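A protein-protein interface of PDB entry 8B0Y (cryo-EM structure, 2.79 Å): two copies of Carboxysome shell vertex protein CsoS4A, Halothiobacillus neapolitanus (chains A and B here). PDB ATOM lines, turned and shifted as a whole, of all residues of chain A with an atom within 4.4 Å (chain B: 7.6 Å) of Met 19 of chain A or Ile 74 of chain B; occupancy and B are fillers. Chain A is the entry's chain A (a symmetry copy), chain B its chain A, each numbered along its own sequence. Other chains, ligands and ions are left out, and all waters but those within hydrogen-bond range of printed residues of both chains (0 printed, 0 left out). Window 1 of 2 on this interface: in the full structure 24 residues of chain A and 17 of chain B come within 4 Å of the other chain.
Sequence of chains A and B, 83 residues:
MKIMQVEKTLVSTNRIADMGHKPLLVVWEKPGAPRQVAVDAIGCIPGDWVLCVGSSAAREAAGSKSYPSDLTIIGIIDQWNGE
No position is printed for both chains. Of the 12 pairs that touch across the chains among the printed residues, none has its exchanged pair printed and touching as well.
Of the 11 printed residues of chain A, 7 touch a printed residue of chain B. Printed residues of chain A that touch a printed residue of chain B: Arg 15, Ile 16, Asp 18, Met 19, Leu 24, Tyr 67 and Pro 68. Of the 23 printed residues of chain B, 8 touch a printed residue of chain A. Printed residues of chain B that touch a printed residue of chain A: Met 1, Ile 42, Leu 51, Val 53, Ala 57, Glu 60, Ile 74 and Gly 75. Along chain B the printed residues that touch a printed residue of chain A span positions 1 to 75. Among the printed residues, 12 pairs touch across the chains. Among the printed residues, no Asp or Glu carboxylate lies within 4 Å of a Lys or Arg side-chain nitrogen of the other chain.
The backbone NH (N) of Ile 16 of chain A lies within hydrogen-bond range of the backbone carbonyl oxygen (O) of Ile 74 of chain B, 3.1 Å away.
Ile 74 of chain B touches Arg 15 of chain A (O to CA, 3.3 Å). Gly 75 of chain B touches Arg 15 of chain A. Ile 16 of chain A touches Ile 42 of chain B. Asp 18 of chain A touches Glu 60 of chain B (OD2 to O, 3.9 Å). Met 1 of chain B touches Met 19 of chain A (CE to CE, 3.9 Å). Ile 74 of chain B touches Met 19 of chain A (CD1 to SD, 3.6 Å). CD2 of Leu 24 of chain A touches CE of Met 1 of chain B, 3.5 Å away. O of Tyr 67 of chain A touches CB of Ala 57 of chain B, 3.99 Å away. Pro 68 of chain A touches Val 53 of chain B. Pro 68 of chain A touches Ala 57 of chain B.
The backbone carbonyl oxygen of Thr 72 of chain B is in hydrogen-bond range of the backbone NH of Val 53 of chain B, 2.9 Å away. The guanidinium group of Arg 15 of chain A sits at hydrogen-bond distance from the backbone carbonyl oxygen of Lys 22 of chain A (3.1 Å). O of Gly 75 of chain B is in hydrogen-bond range of N of Leu 51 of chain B (2.6 Å). The guanidinium group (NH2) of Arg 15 of chain A sits at hydrogen-bond distance from the backbone carbonyl oxygen (O) of Gly 20 of chain A (2.7 Å). The backbone NH (N) of Ile 42 of chain B lies close to the side-chain carboxylate (OD1) of Asp 40 of chain B (3.4 Å). The backbone carbonyl oxygen of Leu 51 of chain B lies within hydrogen-bond range of the backbone NH of Ile 74 of chain B (2.7 Å).
Of the printed residues of chain B, Ile 16 of chain A touches Ile 42 and Ile 74. Printed residues of chain B within 4 Å of Asp 18 of chain A: Glu 60 (3.9 Å). Of chain B, only Met 1 and Ile 74 come within 4 Å of Met 19 of chain A. No residue of chain B comes within 4 Å of Gly 20 of chain A. Of the printed residues of chain B, Pro 68 of chain A touches Val 53 and Ala 57. Val 39 of chain B touches none of the printed residues of chain A. Of chain A, only Arg 15 (3.3 Å), Ile 16 (3.1 Å) and Met 19 (3.6 Å) come within 4 Å of Ile 74 of chain B. The nearest residue of chain B that does not touch Met 19 of chain A is Leu 51 of chain B (4.6 Å). The nearest residue of chain A that does not touch Ile 74 of chain B is Pro 68 of chain A (4.1 Å).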
ATOM      1  N   ARG A  15      -8.838 -19.603   2.927  1.00  0.00           N
ATOM      2  CA  ARG A  15      -9.203 -19.958   4.287  1.00  0.00           C
ATOM      3  C   ARG A  15      -8.739 -21.380   4.566  1.00  0.00           C
ATOM      4  O   ARG A  15      -8.514 -22.172   3.647  1.00  0.00           O
ATOM      5  CB  ARG A  15     -10.715 -19.822   4.513  1.00  0.00           C
ATOM      6  CG  ARG A  15     -11.554 -20.858   3.796  1.00  0.00           C
ATOM      7  CD  ARG A  15     -13.035 -20.626   4.044  1.00  0.00           C
ATOM      8  NE  ARG A  15     -13.834 -21.784   3.666  1.00  0.00           N
ATOM      9  CZ  ARG A  15     -15.157 -21.838   3.735  1.00  0.00           C
ATOM     10  NH1 ARG A  15     -15.870 -20.810   4.161  1.00  0.00           N
ATOM     11  NH2 ARG A  15     -15.779 -22.953   3.367  1.00  0.00           N
ATOM     12  N   ILE A  16      -8.573 -21.692   5.854  1.00  0.00           N
ATOM     13  CA  ILE A  16      -8.017 -22.985   6.228  1.00  0.00           C
ATOM     14  C   ILE A  16      -8.943 -24.106   5.767  1.00  0.00           C
ATOM     15  O   ILE A  16     -10.168 -23.947   5.685  1.00  0.00           O
ATOM     16  CB  ILE A  16      -7.767 -23.061   7.744  1.00  0.00           C
ATOM     17  CG1 ILE A  16      -9.076 -22.908   8.518  1.00  0.00           C
ATOM     18  CG2 ILE A  16      -6.765 -22.003   8.171  1.00  0.00           C
ATOM     19  CD1 ILE A  16      -8.941 -23.150  10.000  1.00  0.00           C
ATOM     20  N   ALA A  17      -8.346 -25.255   5.449  1.00  0.00           N
ATOM     21  CA  ALA A  17      -9.097 -26.390   4.926  1.00  0.00           C
ATOM     22  C   ALA A  17     -10.029 -27.010   5.956  1.00  0.00           C
ATOM     23  O   ALA A  17     -10.889 -27.813   5.580  1.00  0.00           O
ATOM     24  CB  ALA A  17      -8.136 -27.452   4.393  1.00  0.00           C
ATOM     25  N   ASP A  18      -9.881 -26.666   7.237  1.00  0.00           N
ATOM     26  CA  ASP A  18     -10.762 -27.209   8.263  1.00  0.00           C
ATOM     27  C   ASP A  18     -12.176 -26.652   8.169  1.00  0.00           C
ATOM     28  O   ASP A  18     -13.101 -27.255   8.723  1.00  0.00           O
ATOM     29  CB  ASP A  18     -10.188 -26.930   9.650  1.00  0.00           C
ATOM     30  CG  ASP A  18      -8.916 -27.703   9.918  1.00  0.00           C
ATOM     31  OD1 ASP A  18      -8.600 -28.621   9.133  1.00  0.00           O
ATOM     32  OD2 ASP A  18      -8.230 -27.393  10.915  1.00  0.00           O
ATOM     33  N   MET A  19     -12.367 -25.522   7.487  1.00  0.00           N
ATOM     34  CA  MET A  19     -13.699 -24.947   7.345  1.00  0.00           C
ATOM     35  C   MET A  19     -14.564 -25.696   6.343  1.00  0.00           C
ATOM     36  O   MET A  19     -15.766 -25.420   6.267  1.00  0.00           O
ATOM     37  CB  MET A  19     -13.602 -23.479   6.934  1.00  0.00           C
ATOM     38  CG  MET A  19     -12.522 -22.700   7.652  1.00  0.00           C
ATOM     39  SD  MET A  19     -12.928 -20.952   7.806  1.00  0.00           S
ATOM     40  CE  MET A  19     -14.604 -21.053   8.424  1.00  0.00           C
ATOM     41  N   GLY A  20     -13.993 -26.625   5.580  1.00  0.00           N
ATOM     42  CA  GLY A  20     -14.777 -27.373   4.624  1.00  0.00           C
ATOM     43  C   GLY A  20     -15.371 -26.475   3.554  1.00  0.00           C
ATOM     44  O   GLY A  20     -14.770 -25.492   3.114  1.00  0.00           O
ATOM     45  N   HIS A  21     -16.585 -26.825   3.132  1.00  0.00           N
ATOM     46  CA  HIS A  21     -17.308 -26.080   2.111  1.00  0.00           C
ATOM     47  C   HIS A  21     -18.485 -25.300   2.681  1.00  0.00           C
ATOM     48  O   HIS A  21     -19.370 -24.891   1.923  1.00  0.00           O
ATOM     49  CB  HIS A  21     -17.789 -27.031   1.014  1.00  0.00           C
ATOM     50  CG  HIS A  21     -16.808 -28.110   0.677  1.00  0.00           C
ATOM     51  ND1 HIS A  21     -15.823 -27.951  -0.274  1.00  0.00           N
ATOM     52  CD2 HIS A  21     -16.657 -29.363   1.166  1.00  0.00           C
ATOM     53  CE1 HIS A  21     -15.110 -29.060  -0.357  1.00  0.00           C
ATOM     54  NE2 HIS A  21     -15.596 -29.932   0.506  1.00  0.00           N
ATOM     55  N   LYS A  22     -18.518 -25.084   3.992  1.00  0.00           N
ATOM     56  CA  LYS A  22     -19.657 -24.420   4.611  1.00  0.00           C
ATOM     57  C   LYS A  22     -19.686 -22.942   4.228  1.00  0.00           C
ATOM     58  O   LYS A  22     -18.641 -22.286   4.190  1.00  0.00           O
ATOM     59  CB  LYS A  22     -19.596 -24.563   6.130  1.00  0.00           C
ATOM     60  CG  LYS A  22     -19.525 -25.999   6.619  1.00  0.00           C
ATOM     61  CD  LYS A  22     -20.828 -26.736   6.377  1.00  0.00           C
ATOM     62  CE  LYS A  22     -21.909 -26.280   7.342  1.00  0.00           C
ATOM     63  NZ  LYS A  22     -23.153 -27.083   7.204  1.00  0.00           N
ATOM     64  N   LEU A  24     -20.350 -18.844   4.563  1.00  0.00           N
ATOM     65  CA  LEU A  24     -20.141 -17.840   5.595  1.00  0.00           C
ATOM     66  C   LEU A  24     -21.064 -16.657   5.344  1.00  0.00           C
ATOM     67  O   LEU A  24     -21.180 -16.180   4.211  1.00  0.00           O
ATOM     68  CB  LEU A  24     -18.685 -17.367   5.625  1.00  0.00           C
ATOM     69  CG  LEU A  24     -17.631 -18.434   5.917  1.00  0.00           C
ATOM     70  CD1 LEU A  24     -16.238 -17.840   5.815  1.00  0.00           C
ATOM     71  CD2 LEU A  24     -17.858 -19.048   7.287  1.00  0.00           C
ATOM     72  N   TYR A  67     -14.731 -28.544  14.190  1.00  0.00           N
ATOM     73  CA  TYR A  67     -14.890 -27.497  13.194  1.00  0.00           C
ATOM     74  C   TYR A  67     -14.444 -26.149  13.763  1.00  0.00           C
ATOM     75  O   TYR A  67     -14.768 -25.820  14.908  1.00  0.00           O
ATOM     76  CB  TYR A  67     -16.342 -27.412  12.728  1.00  0.00           C
ATOM     77  CG  TYR A  67     -16.519 -26.623  11.455  1.00  0.00           C
ATOM     78  CD1 TYR A  67     -16.725 -25.252  11.490  1.00  0.00           C
ATOM     79  CD2 TYR A  67     -16.472 -27.245  10.218  1.00  0.00           C
ATOM     80  CE1 TYR A  67     -16.882 -24.524  10.333  1.00  0.00           C
ATOM     81  CE2 TYR A  67     -16.629 -26.524   9.054  1.00  0.00           C
ATOM     82  CZ  TYR A  67     -16.833 -25.163   9.118  1.00  0.00           C
ATOM     83  OH  TYR A  67     -16.990 -24.436   7.963  1.00  0.00           O
ATOM     84  N   PRO A  68     -13.705 -25.349  12.990  1.00  0.00           N
ATOM     85  CA  PRO A  68     -13.237 -24.029  13.467  1.00  0.00           C
ATOM     86  C   PRO A  68     -14.311 -22.953  13.352  1.00  0.00           C
ATOM     87  O   PRO A  68     -14.244 -22.029  12.535  1.00  0.00           O
ATOM     88  CB  PRO A  68     -12.035 -23.763  12.558  1.00  0.00           C
ATOM     89  CG  PRO A  68     -12.395 -24.441  11.283  1.00  0.00           C
ATOM     90  CD  PRO A  68     -13.165 -25.678  11.658  1.00  0.00           C
ATOM     91  N   MET B   1     -17.220 -15.554  14.975  1.00  0.00           N
ATOM     92  CA  MET B   1     -16.189 -15.107  14.047  1.00  0.00           C
ATOM     93  C   MET B   1     -16.376 -13.632  13.716  1.00  0.00           C
ATOM     94  O   MET B   1     -17.495 -13.176  13.494  1.00  0.00           O
ATOM     95  CB  MET B   1     -16.215 -15.951  12.773  1.00  0.00           C
ATOM     96  CG  MET B   1     -16.009 -17.437  13.020  1.00  0.00           C
ATOM     97  SD  MET B   1     -17.265 -18.468  12.242  1.00  0.00           S
ATOM     98  CE  MET B   1     -16.637 -18.558  10.569  1.00  0.00           C
ATOM     99  N   LYS B   2     -15.275 -12.887  13.689  1.00  0.00           N
ATOM    100  CA  LYS B   2     -15.306 -11.453  13.452  1.00  0.00           C
ATOM    101  C   LYS B   2     -14.336 -11.098  12.336  1.00  0.00           C
ATOM    102  O   LYS B   2     -13.584 -11.940  11.840  1.00  0.00           O
ATOM    103  CB  LYS B   2     -14.965 -10.668  14.725  1.00  0.00           C
ATOM    104  CG  LYS B   2     -16.115 -10.554  15.707  1.00  0.00           C
ATOM    105  CD  LYS B   2     -15.723  -9.737  16.921  1.00  0.00           C
ATOM    106  CE  LYS B   2     -16.174 -10.411  18.204  1.00  0.00           C
ATOM    107  NZ  LYS B   2     -15.928 -11.878  18.170  1.00  0.00           N
ATOM    108  N   ALA B  38      -3.407 -12.450  17.648  1.00  0.00           N
ATOM    109  CA  ALA B  38      -3.974 -13.656  17.066  1.00  0.00           C
ATOM    110  C   ALA B  38      -2.872 -14.504  16.452  1.00  0.00           C
ATOM    111  O   ALA B  38      -1.856 -13.987  15.982  1.00  0.00           O
ATOM    112  CB  ALA B  38      -5.026 -13.326  16.003  1.00  0.00           C
ATOM    113  N   VAL B  39      -3.084 -15.815  16.465  1.00  0.00           N
ATOM    114  CA  VAL B  39      -2.170 -16.741  15.807  1.00  0.00           C
ATOM    115  C   VAL B  39      -2.435 -16.704  14.309  1.00  0.00           C
ATOM    116  O   VAL B  39      -3.577 -16.863  13.861  1.00  0.00           O
ATOM    117  CB  VAL B  39      -2.335 -18.162  16.369  1.00  0.00           C
ATOM    118  CG1 VAL B  39      -1.767 -19.186  15.402  1.00  0.00           C
ATOM    119  CG2 VAL B  39      -1.660 -18.275  17.723  1.00  0.00           C
ATOM    120  N   ASP B  40      -1.380 -16.489  13.527  1.00  0.00           N
ATOM    121  CA  ASP B  40      -1.492 -16.382  12.074  1.00  0.00           C
ATOM    122  C   ASP B  40      -1.409 -17.781  11.478  1.00  0.00           C
ATOM    123  O   ASP B  40      -0.318 -18.320  11.275  1.00  0.00           O
ATOM    124  CB  ASP B  40      -0.403 -15.472  11.522  1.00  0.00           C
ATOM    125  CG  ASP B  40      -0.643 -15.088  10.080  1.00  0.00           C
ATOM    126  OD1 ASP B  40      -1.752 -15.349   9.570  1.00  0.00           O
ATOM    127  OD2 ASP B  40       0.278 -14.517   9.458  1.00  0.00           O
ATOM    128  N   ALA B  41      -2.566 -18.374  11.197  1.00  0.00           N
ATOM    129  CA  ALA B  41      -2.633 -19.692  10.582  1.00  0.00           C
ATOM    130  C   ALA B  41      -2.695 -19.632   9.062  1.00  0.00           C
ATOM    131  O   ALA B  41      -2.693 -20.685   8.415  1.00  0.00           O
ATOM    132  CB  ALA B  41      -3.846 -20.463  11.114  1.00  0.00           C
ATOM    133  N   ILE B  42      -2.748 -18.436   8.481  1.00  0.00           N
ATOM    134  CA  ILE B  42      -2.849 -18.250   7.039  1.00  0.00           C
ATOM    135  C   ILE B  42      -1.593 -17.603   6.471  1.00  0.00           C
ATOM    136  O   ILE B  42      -1.006 -18.100   5.504  1.00  0.00           O
ATOM    137  CB  ILE B  42      -4.103 -17.426   6.665  1.00  0.00           C
ATOM    138  CG1 ILE B  42      -5.371 -18.242   6.909  1.00  0.00           C
ATOM    139  CG2 ILE B  42      -4.034 -16.965   5.221  1.00  0.00           C
ATOM    140  CD1 ILE B  42      -5.534 -19.411   5.968  1.00  0.00           C
ATOM    141  N   VAL B  50      -9.000  -9.751   7.648  1.00  0.00           N
ATOM    142  CA  VAL B  50      -8.892 -11.184   7.868  1.00  0.00           C
ATOM    143  C   VAL B  50     -10.093 -11.678   8.659  1.00  0.00           C
ATOM    144  O   VAL B  50     -10.831 -10.905   9.272  1.00  0.00           O
ATOM    145  CB  VAL B  50      -7.584 -11.562   8.594  1.00  0.00           C
ATOM    146  CG1 VAL B  50      -6.389 -11.302   7.699  1.00  0.00           C
ATOM    147  CG2 VAL B  50      -7.457 -10.791   9.894  1.00  0.00           C
ATOM    148  N   LEU B  51     -10.275 -12.993   8.635  1.00  0.00           N
ATOM    149  CA  LEU B  51     -11.337 -13.663   9.371  1.00  0.00           C
ATOM    150  C   LEU B  51     -10.725 -14.340  10.592  1.00  0.00           C
ATOM    151  O   LEU B  51      -9.776 -15.118  10.463  1.00  0.00           O
ATOM    152  CB  LEU B  51     -12.050 -14.681   8.481  1.00  0.00           C
ATOM    153  CG  LEU B  51     -13.362 -15.262   9.005  1.00  0.00           C
ATOM    154  CD1 LEU B  51     -14.444 -14.198   9.021  1.00  0.00           C
ATOM    155  CD2 LEU B  51     -13.788 -16.447   8.159  1.00  0.00           C
ATOM    156  N   CYS B  52     -11.263 -14.040  11.770  1.00  0.00           N
ATOM    157  CA  CYS B  52     -10.732 -14.549  13.025  1.00  0.00           C
ATOM    158  C   CYS B  52     -11.749 -15.460  13.694  1.00  0.00           C
ATOM    159  O   CYS B  52     -12.960 -15.287  13.527  1.00  0.00           O
ATOM    160  CB  CYS B  52     -10.362 -13.409  13.978  1.00  0.00           C
ATOM    161  SG  CYS B  52     -11.775 -12.625  14.777  1.00  0.00           S
ATOM    162  N   VAL B  53     -11.248 -16.435  14.445  1.00  0.00           N
ATOM    163  CA  VAL B  53     -12.082 -17.323  15.243  1.00  0.00           C
ATOM    164  C   VAL B  53     -11.530 -17.349  16.662  1.00  0.00           C
ATOM    165  O   VAL B  53     -10.326 -17.198  16.885  1.00  0.00           O
ATOM    166  CB  VAL B  53     -12.157 -18.745  14.641  1.00  0.00           C
ATOM    167  CG1 VAL B  53     -10.863 -19.509  14.878  1.00  0.00           C
ATOM    168  CG2 VAL B  53     -13.347 -19.502  15.201  1.00  0.00           C
ATOM    169  N   GLY B  54     -12.429 -17.511  17.628  1.00  0.00           N
ATOM    170  CA  GLY B  54     -12.039 -17.560  19.022  1.00  0.00           C
ATOM    171  C   GLY B  54     -12.511 -18.818  19.717  1.00  0.00           C
ATOM    172  O   GLY B  54     -12.805 -19.821  19.060  1.00  0.00           O
ATOM    173  N   ALA B  57     -12.371 -23.167  19.176  1.00  0.00           N
ATOM    174  CA  ALA B  57     -12.105 -23.366  17.757  1.00  0.00           C
ATOM    175  C   ALA B  57     -10.753 -22.783  17.366  1.00  0.00           C
ATOM    176  O   ALA B  57     -10.069 -23.317  16.482  1.00  0.00           O
ATOM    177  CB  ALA B  57     -13.222 -22.744  16.923  1.00  0.00           C
ATOM    178  N   ALA B  58     -10.354 -21.685  18.011  1.00  0.00           N
ATOM    179  CA  ALA B  58      -9.065 -21.069  17.726  1.00  0.00           C
ATOM    180  C   ALA B  58      -7.897 -21.968  18.105  1.00  0.00           C
ATOM    181  O   ALA B  58      -6.801 -21.801  17.562  1.00  0.00           O
ATOM    182  CB  ALA B  58      -8.951 -19.734  18.457  1.00  0.00           C
ATOM    183  N   GLU B  60      -7.716 -25.520  17.747  1.00  0.00           N
ATOM    184  CA  GLU B  60      -7.491 -26.461  16.658  1.00  0.00           C
ATOM    185  C   GLU B  60      -7.301 -25.762  15.321  1.00  0.00           C
ATOM    186  O   GLU B  60      -6.754 -26.367  14.393  1.00  0.00           O
ATOM    187  CB  GLU B  60      -8.648 -27.455  16.573  1.00  0.00           C
ATOM    188  CG  GLU B  60      -8.213 -28.877  16.264  1.00  0.00           C
ATOM    189  CD  GLU B  60      -9.323 -29.886  16.471  1.00  0.00           C
ATOM    190  OE1 GLU B  60     -10.001 -29.818  17.518  1.00  0.00           O
ATOM    191  OE2 GLU B  60      -9.516 -30.749  15.590  1.00  0.00           O
ATOM    192  N   ALA B  61      -7.740 -24.507  15.195  1.00  0.00           N
ATOM    193  CA  ALA B  61      -7.444 -23.749  13.986  1.00  0.00           C
ATOM    194  C   ALA B  61      -5.973 -23.374  13.914  1.00  0.00           C
ATOM    195  O   ALA B  61      -5.445 -23.133  12.823  1.00  0.00           O
ATOM    196  CB  ALA B  61      -8.320 -22.499  13.921  1.00  0.00           C
ATOM    197  N   ALA B  62      -5.295 -23.320  15.061  1.00  0.00           N
ATOM    198  CA  ALA B  62      -3.877 -22.994  15.107  1.00  0.00           C
ATOM    199  C   ALA B  62      -2.979 -24.213  14.947  1.00  0.00           C
ATOM    200  O   ALA B  62      -1.754 -24.057  14.924  1.00  0.00           O
ATOM    201  CB  ALA B  62      -3.543 -22.283  16.419  1.00  0.00           C
ATOM    202  N   LEU B  71      -7.497 -16.897  19.877  1.00  0.00           N
ATOM    203  CA  LEU B  71      -7.800 -16.064  18.718  1.00  0.00           C
ATOM    204  C   LEU B  71      -6.858 -16.471  17.600  1.00  0.00           C
ATOM    205  O   LEU B  71      -5.638 -16.376  17.757  1.00  0.00           O
ATOM    206  CB  LEU B  71      -7.646 -14.579  19.048  1.00  0.00           C
ATOM    207  CG  LEU B  71      -8.215 -13.599  18.020  1.00  0.00           C
ATOM    208  CD1 LEU B  71      -9.709 -13.798  17.859  1.00  0.00           C
ATOM    209  CD2 LEU B  71      -7.905 -12.166  18.410  1.00  0.00           C
ATOM    210  N   THR B  72      -7.415 -16.934  16.483  1.00  0.00           N
ATOM    211  CA  THR B  72      -6.631 -17.388  15.345  1.00  0.00           C
ATOM    212  C   THR B  72      -7.210 -16.800  14.067  1.00  0.00           C
ATOM    213  O   THR B  72      -8.431 -16.691  13.923  1.00  0.00           O
ATOM    214  CB  THR B  72      -6.612 -18.923  15.258  1.00  0.00           C
ATOM    215  OG1 THR B  72      -6.147 -19.466  16.499  1.00  0.00           O
ATOM    216  CG2 THR B  72      -5.694 -19.393  14.145  1.00  0.00           C
ATOM    217  N   ILE B  73      -6.331 -16.424  13.144  1.00  0.00           N
ATOM    218  CA  ILE B  73      -6.750 -15.937  11.834  1.00  0.00           C
ATOM    219  C   ILE B  73      -6.926 -17.137  10.912  1.00  0.00           C
ATOM    220  O   ILE B  73      -5.975 -17.888  10.668  1.00  0.00           O
ATOM    221  CB  ILE B  73      -5.734 -14.940  11.263  1.00  0.00           C
ATOM    222  CG1 ILE B  73      -5.697 -13.674  12.118  1.00  0.00           C
ATOM    223  CG2 ILE B  73      -6.068 -14.613   9.821  1.00  0.00           C
ATOM    224  CD1 ILE B  73      -4.416 -12.886  11.984  1.00  0.00           C
ATOM    225  N   ILE B  74      -8.140 -17.320  10.397  1.00  0.00           N
ATOM    226  CA  ILE B  74      -8.490 -18.509   9.628  1.00  0.00           C
ATOM    227  C   ILE B  74      -8.775 -18.206   8.170  1.00  0.00           C
ATOM    228  O   ILE B  74      -9.208 -19.107   7.438  1.00  0.00           O
ATOM    229  CB  ILE B  74      -9.685 -19.249  10.257  1.00  0.00           C
ATOM    230  CG1 ILE B  74     -10.866 -18.297  10.443  1.00  0.00           C
ATOM    231  CG2 ILE B  74      -9.282 -19.873  11.578  1.00  0.00           C
ATOM    232  CD1 ILE B  74     -12.176 -18.999  10.699  1.00  0.00           C
ATOM    233  N   GLY B  75      -8.556 -16.980   7.719  1.00  0.00           N
ATOM    234  CA  GLY B  75      -8.752 -16.672   6.318  1.00  0.00           C
ATOM    235  C   GLY B  75      -8.624 -15.188   6.066  1.00  0.00           C
ATOM    236  O   GLY B  75      -8.756 -14.364   6.977  1.00  0.00           O
ATOM    237  N   ILE B  76      -8.363 -14.864   4.804  1.00  0.00           N
ATOM    238  CA  ILE B  76      -8.296 -13.490   4.322  1.00  0.00           C
ATOM    239  C   ILE B  76      -9.525 -13.240   3.462  1.00  0.00           C
ATOM    240  O   ILE B  76      -9.823 -14.024   2.553  1.00  0.00           O
ATOM    241  CB  ILE B  76      -7.008 -13.232   3.523  1.00  0.00           C
ATOM    242  CG1 ILE B  76      -5.777 -13.526   4.378  1.00  0.00           C
ATOM    243  CG2 ILE B  76      -6.971 -11.799   3.026  1.00  0.00           C
ATOM    244  CD1 ILE B  76      -4.473 -13.306   3.652  1.00  0.00           C
